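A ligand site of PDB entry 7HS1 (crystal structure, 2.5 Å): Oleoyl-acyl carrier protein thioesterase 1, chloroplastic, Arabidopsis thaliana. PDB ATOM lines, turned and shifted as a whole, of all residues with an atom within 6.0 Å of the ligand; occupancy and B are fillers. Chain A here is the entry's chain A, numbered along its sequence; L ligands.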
ATOM      1  N   GLY A  41      11.151  14.411 -32.635  1.00  0.00           N
ATOM      2  CA  GLY A  41      10.466  15.646 -32.247  1.00  0.00           C
ATOM      3  C   GLY A  41       9.087  15.376 -31.657  1.00  0.00           C
ATOM      4  O   GLY A  41       8.633  16.116 -30.786  1.00  0.00           O
ATOM      5  N   HIS A  44       9.752  13.946 -28.087  1.00  0.00           N
ATOM      6  CA  HIS A  44      10.167  15.044 -27.218  1.00  0.00           C
ATOM      7  C   HIS A  44       8.929  15.812 -26.715  1.00  0.00           C
ATOM      8  O   HIS A  44       8.862  16.156 -25.544  1.00  0.00           O
ATOM      9  CB  HIS A  44      11.125  15.992 -27.971  1.00  0.00           C
ATOM     10  CG  HIS A  44      11.702  17.078 -27.127  1.00  0.00           C
ATOM     11  ND1 HIS A  44      12.291  18.184 -27.696  1.00  0.00           N
ATOM     12  CD2 HIS A  44      11.766  17.209 -25.772  1.00  0.00           C
ATOM     13  CE1 HIS A  44      12.707  18.934 -26.693  1.00  0.00           C
ATOM     14  NE2 HIS A  44      12.392  18.396 -25.517  1.00  0.00           N
ATOM     15  N   ALA A  45       7.938  16.076 -27.592  1.00  0.00           N
ATOM     16  CA  ALA A  45       6.709  16.777 -27.191  1.00  0.00           C
ATOM     17  C   ALA A  45       5.881  15.928 -26.211  1.00  0.00           C
ATOM     18  O   ALA A  45       5.382  16.453 -25.229  1.00  0.00           O
ATOM     19  CB  ALA A  45       5.883  17.125 -28.415  1.00  0.00           C
ATOM     20  N   GLN A  46       5.796  14.613 -26.452  1.00  0.00           N
ATOM     21  CA  GLN A  46       5.054  13.691 -25.613  1.00  0.00           C
ATOM     22  C   GLN A  46       5.693  13.556 -24.225  1.00  0.00           C
ATOM     23  O   GLN A  46       4.994  13.428 -23.223  1.00  0.00           O
ATOM     24  CB  GLN A  46       5.002  12.321 -26.283  1.00  0.00           C
ATOM     25  CG  GLN A  46       3.595  11.825 -26.547  1.00  0.00           C
ATOM     26  CD  GLN A  46       3.563  10.315 -26.732  1.00  0.00           C
ATOM     27  OE1 GLN A  46       3.524   9.793 -27.872  1.00  0.00           O
ATOM     28  NE2 GLN A  46       3.572   9.578 -25.617  1.00  0.00           N
ATOM     29  N   VAL A  48       7.154  15.770 -22.464  1.00  0.00           N
ATOM     30  CA  VAL A  48       6.948  16.931 -21.602  1.00  0.00           C
ATOM     31  C   VAL A  48       5.505  17.430 -21.537  1.00  0.00           C
ATOM     32  O   VAL A  48       5.273  18.543 -21.057  1.00  0.00           O
ATOM     33  CB  VAL A  48       7.891  18.104 -21.941  1.00  0.00           C
ATOM     34  CG1 VAL A  48       9.338  17.724 -21.670  1.00  0.00           C
ATOM     35  CG2 VAL A  48       7.709  18.542 -23.380  1.00  0.00           C
ATOM     36  N   PHE A  50       2.654  17.393 -24.209  1.00  0.00           N
ATOM     37  CA  PHE A  50       2.091  18.038 -25.384  1.00  0.00           C
ATOM     38  C   PHE A  50       1.297  17.011 -26.210  1.00  0.00           C
ATOM     39  O   PHE A  50       1.332  15.810 -25.893  1.00  0.00           O
ATOM     40  CB  PHE A  50       3.199  18.682 -26.241  1.00  0.00           C
ATOM     41  CG  PHE A  50       3.785  19.941 -25.653  1.00  0.00           C
ATOM     42  CD1 PHE A  50       2.973  21.010 -25.336  1.00  0.00           C
ATOM     43  CD2 PHE A  50       5.140  20.059 -25.438  1.00  0.00           C
ATOM     44  CE1 PHE A  50       3.518  22.169 -24.771  1.00  0.00           C
ATOM     45  CE2 PHE A  50       5.681  21.209 -24.875  1.00  0.00           C
ATOM     46  CZ  PHE A  50       4.859  22.259 -24.550  1.00  0.00           C
ATOM     47  N   ALA A  56       2.291  19.758 -31.460  1.00  0.00           N
ATOM     48  CA  ALA A  56       2.832  20.093 -30.150  1.00  0.00           C
ATOM     49  C   ALA A  56       2.044  21.258 -29.563  1.00  0.00           C
ATOM     50  O   ALA A  56       2.607  22.305 -29.203  1.00  0.00           O
ATOM     51  CB  ALA A  56       4.312  20.433 -30.272  1.00  0.00           C
ATOM     52  N   TRP A  68       0.904  24.497 -34.829  1.00  0.00           N
ATOM     53  CA  TRP A  68       2.235  24.887 -35.256  1.00  0.00           C
ATOM     54  C   TRP A  68       2.430  24.296 -36.640  1.00  0.00           C
ATOM     55  O   TRP A  68       2.172  23.104 -36.828  1.00  0.00           O
ATOM     56  CB  TRP A  68       3.303  24.286 -34.326  1.00  0.00           C
ATOM     57  CG  TRP A  68       3.390  24.923 -32.972  1.00  0.00           C
ATOM     58  CD1 TRP A  68       2.993  24.387 -31.789  1.00  0.00           C
ATOM     59  CD2 TRP A  68       3.948  26.211 -32.674  1.00  0.00           C
ATOM     60  NE1 TRP A  68       3.294  25.249 -30.756  1.00  0.00           N
ATOM     61  CE2 TRP A  68       3.843  26.398 -31.275  1.00  0.00           C
ATOM     62  CE3 TRP A  68       4.528  27.226 -33.435  1.00  0.00           C
ATOM     63  CZ2 TRP A  68       4.300  27.541 -30.633  1.00  0.00           C
ATOM     64  CZ3 TRP A  68       4.979  28.373 -32.805  1.00  0.00           C
ATOM     65  CH2 TRP A  68       4.861  28.524 -31.421  1.00  0.00           C
ATOM     66  N   CYS A  93      14.190  22.453 -28.893  1.00  0.00           N
ATOM     67  CA  CYS A  93      13.433  23.550 -29.456  1.00  0.00           C
ATOM     68  C   CYS A  93      13.883  24.863 -28.825  1.00  0.00           C
ATOM     69  O   CYS A  93      14.404  24.884 -27.721  1.00  0.00           O
ATOM     70  CB  CYS A  93      11.940  23.305 -29.254  1.00  0.00           C
ATOM     71  SG  CYS A  93      10.871  24.538 -30.055  1.00  0.00           S
ATOM     72  N   THR A 101       8.797  29.390 -33.356  1.00  0.00           N
ATOM     73  CA  THR A 101       9.792  28.498 -32.805  1.00  0.00           C
ATOM     74  C   THR A 101      10.763  27.955 -33.865  1.00  0.00           C
ATOM     75  O   THR A 101      10.506  28.051 -35.057  1.00  0.00           O
ATOM     76  CB  THR A 101       9.111  27.368 -32.001  1.00  0.00           C
ATOM     77  OG1 THR A 101       8.198  26.682 -32.850  1.00  0.00           O
ATOM     78  CG2 THR A 101       8.410  27.882 -30.777  1.00  0.00           C
ATOM     79  N   ARG A 102      11.870  27.389 -33.404  1.00  0.00           N
ATOM     80  CA  ARG A 102      12.870  26.758 -34.237  1.00  0.00           C
ATOM     81  C   ARG A 102      13.203  25.404 -33.583  1.00  0.00           C
ATOM     82  O   ARG A 102      13.463  25.371 -32.379  1.00  0.00           O
ATOM     83  CB  ARG A 102      14.114  27.644 -34.312  1.00  0.00           C
ATOM     84  CG  ARG A 102      15.092  27.209 -35.380  1.00  0.00           C
ATOM     85  CD  ARG A 102      16.483  27.770 -35.152  1.00  0.00           C
ATOM     86  NE  ARG A 102      17.093  27.262 -33.920  1.00  0.00           N
ATOM     87  CZ  ARG A 102      17.594  28.023 -32.953  1.00  0.00           C
ATOM     88  NH1 ARG A 102      18.116  27.475 -31.873  1.00  0.00           N
ATOM     89  NH2 ARG A 102      17.566  29.346 -33.059  1.00  0.00           N
ATOM     90  N   ARG A 103      13.140  24.293 -34.348  1.00  0.00           N
ATOM     91  CA  ARG A 103      13.550  22.995 -33.785  1.00  0.00           C
ATOM     92  C   ARG A 103      14.843  22.546 -34.468  1.00  0.00           C
ATOM     93  O   ARG A 103      14.954  22.628 -35.686  1.00  0.00           O
ATOM     94  CB  ARG A 103      12.464  21.904 -33.842  1.00  0.00           C
ATOM     95  CG  ARG A 103      12.991  20.592 -33.234  1.00  0.00           C
ATOM     96  CD  ARG A 103      12.012  19.447 -33.155  1.00  0.00           C
ATOM     97  NE  ARG A 103      11.029  19.588 -32.080  1.00  0.00           N
ATOM     98  CZ  ARG A 103      11.255  19.294 -30.794  1.00  0.00           C
ATOM     99  NH1 ARG A 103      10.290  19.429 -29.901  1.00  0.00           N
ATOM    100  NH2 ARG A 103      12.446  18.878 -30.411  1.00  0.00           N
ATOM    101  N   TRP A 123       9.078  27.114 -37.437  1.00  0.00           N
ATOM    102  CA  TRP A 123       7.662  26.880 -37.326  1.00  0.00           C
ATOM    103  C   TRP A 123       6.908  28.121 -37.001  1.00  0.00           C
ATOM    104  O   TRP A 123       7.303  28.874 -36.118  1.00  0.00           O
ATOM    105  CB  TRP A 123       7.365  25.842 -36.241  1.00  0.00           C
ATOM    106  CG  TRP A 123       8.058  24.536 -36.460  1.00  0.00           C
ATOM    107  CD1 TRP A 123       9.387  24.285 -36.359  1.00  0.00           C
ATOM    108  CD2 TRP A 123       7.431  23.286 -36.736  1.00  0.00           C
ATOM    109  NE1 TRP A 123       9.638  22.959 -36.626  1.00  0.00           N
ATOM    110  CE2 TRP A 123       8.448  22.320 -36.847  1.00  0.00           C
ATOM    111  CE3 TRP A 123       6.102  22.879 -36.925  1.00  0.00           C
ATOM    112  CZ2 TRP A 123       8.188  20.975 -37.119  1.00  0.00           C
ATOM    113  CZ3 TRP A 123       5.841  21.557 -37.197  1.00  0.00           C
ATOM    114  CH2 TRP A 123       6.873  20.614 -37.282  1.00  0.00           C
ATOM    115  N   TYR A 144       5.702  26.906 -23.263  1.00  0.00           N
ATOM    116  CA  TYR A 144       6.750  26.033 -23.759  1.00  0.00           C
ATOM    117  C   TYR A 144       8.167  26.506 -23.451  1.00  0.00           C
ATOM    118  O   TYR A 144       9.105  25.725 -23.615  1.00  0.00           O
ATOM    119  CB  TYR A 144       6.585  25.768 -25.260  1.00  0.00           C
ATOM    120  CG  TYR A 144       6.833  26.976 -26.139  1.00  0.00           C
ATOM    121  CD1 TYR A 144       8.117  27.366 -26.486  1.00  0.00           C
ATOM    122  CD2 TYR A 144       5.773  27.696 -26.669  1.00  0.00           C
ATOM    123  CE1 TYR A 144       8.353  28.489 -27.265  1.00  0.00           C
ATOM    124  CE2 TYR A 144       5.993  28.819 -27.474  1.00  0.00           C
ATOM    125  CZ  TYR A 144       7.279  29.222 -27.768  1.00  0.00           C
ATOM    126  OH  TYR A 144       7.507  30.299 -28.592  1.00  0.00           O
ATOM    127  N   PHE A 147      10.619  24.391 -21.378  1.00  0.00           N
ATOM    128  CA  PHE A 147      11.209  23.178 -21.951  1.00  0.00           C
ATOM    129  C   PHE A 147      12.330  23.478 -22.983  1.00  0.00           C
ATOM    130  O   PHE A 147      12.808  22.569 -23.660  1.00  0.00           O
ATOM    131  CB  PHE A 147      10.097  22.307 -22.578  1.00  0.00           C
ATOM    132  CG  PHE A 147       8.867  22.133 -21.713  1.00  0.00           C
ATOM    133  CD1 PHE A 147       8.948  21.493 -20.493  1.00  0.00           C
ATOM    134  CD2 PHE A 147       7.647  22.650 -22.103  1.00  0.00           C
ATOM    135  CE1 PHE A 147       7.834  21.372 -19.666  1.00  0.00           C
ATOM    136  CE2 PHE A 147       6.529  22.520 -21.278  1.00  0.00           C
ATOM    137  CZ  PHE A 147       6.635  21.882 -20.061  1.00  0.00           C
ATOM    138  N   CYS A 148      12.740  24.754 -23.094  1.00  0.00           N
ATOM    139  CA  CYS A 148      13.738  25.228 -24.047  1.00  0.00           C
ATOM    140  C   CYS A 148      14.921  25.825 -23.328  1.00  0.00           C
ATOM    141  O   CYS A 148      14.720  26.525 -22.330  1.00  0.00           O
ATOM    142  CB  CYS A 148      13.119  26.261 -24.987  1.00  0.00           C
ATOM    143  SG  CYS A 148      11.627  25.697 -25.850  1.00  0.00           S
HETATM  144  C1  LIG L   1       8.469  21.822 -27.831  1.00  0.00           C
HETATM  145  C2  LIG L   1       9.701  20.297 -25.877  1.00  0.00           C
HETATM  146  C3  LIG L   1       9.406  22.389 -26.986  1.00  0.00           C
HETATM  147  C4  LIG L   1       7.125  23.614 -33.529  1.00  0.00           C
HETATM  148  C5  LIG L   1       6.974  22.914 -31.189  1.00  0.00           C
HETATM  149  C6  LIG L   1       6.088  23.999 -30.591  1.00  0.00           C
HETATM  150  C7  LIG L   1       6.872  24.794 -29.561  1.00  0.00           C
HETATM  151  C8  LIG L   1       7.281  23.920 -28.391  1.00  0.00           C
HETATM  152  C9  LIG L   1       7.835  22.194 -30.176  1.00  0.00           C
HETATM  153  C10 LIG L   1       8.144  20.482 -27.684  1.00  0.00           C
HETATM  154  C11 LIG L   1       8.759  19.731 -26.703  1.00  0.00           C
HETATM  155  C12 LIG L   1      10.042  21.620 -26.030  1.00  0.00           C
HETATM  156  N1  LIG L   1       7.839  23.441 -32.265  1.00  0.00           N
HETATM  157  N2  LIG L   1       7.841  22.631 -28.868  1.00  0.00           N
HETATM  158  O1  LIG L   1       8.493  21.231 -30.539  1.00  0.00           O
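SG of Cys 93 sits close to N2 of the ligand (3.8 Å).
His 44 touches the ligand (NE2 to C2, 3.3 Å).
Ala 45 touches the ligand.
Val 48 touches the ligand.
Phe 50 touches the ligand.
Ala 56 touches the ligand.
NE1 of Trp 68 touches C6 of the ligand (3.1 Å).
Trp 123 touches the ligand (CG to C4, 3.2 Å).
Tyr 144 touches the ligand (CB to C8, 3.7 Å).
Phe 147 touches the ligand (CB to C12, 3.5 Å).
Within 4 Å of the ligand: His 44, Ala 45, Val 48, Phe 50, Ala 56, Trp 68, Cys 93, Thr 101, Arg 103, Trp 123, Tyr 144 and Phe 147.
Along chain A the residues within 4 Å of the ligand span positions 44 to 147.
O of Tyr 144 sits at hydrogen-bond distance from SG of Cys 148 (3.4 Å).
A ring nitrogen (ND1) of His 44 is in hydrogen-bond range of the guanidinium group (NH2) of Arg 103, at 2.8 Å.
N of Trp 123 is in hydrogen-bond range of O of Thr 101 (2.9 Å).
NE1 of Trp 68 lies close to O of Ala 56 (3.4 Å).
The backbone carbonyl oxygen (O) of Arg 102 lies close to the side-chain sulfur (SG) of Cys 93 (3.6 Å).
The backbone carbonyl oxygen (O) of Cys 93 sits close to the side-chain sulfur (SG) of Cys 148, 3.4 Å away.
N of Phe 50 sits at hydrogen-bond distance from O of Ala 45, 3.1 Å away.
A nitrogen (N1) of the ligand lies within hydrogen-bond range of the side-chain hydroxyl (OG1) of Thr 101, 3.3 Å away.
An oxygen (O1) of the ligand lies within hydrogen-bond range of the guanidinium group (NH1) of Arg 103 (2.6 Å).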
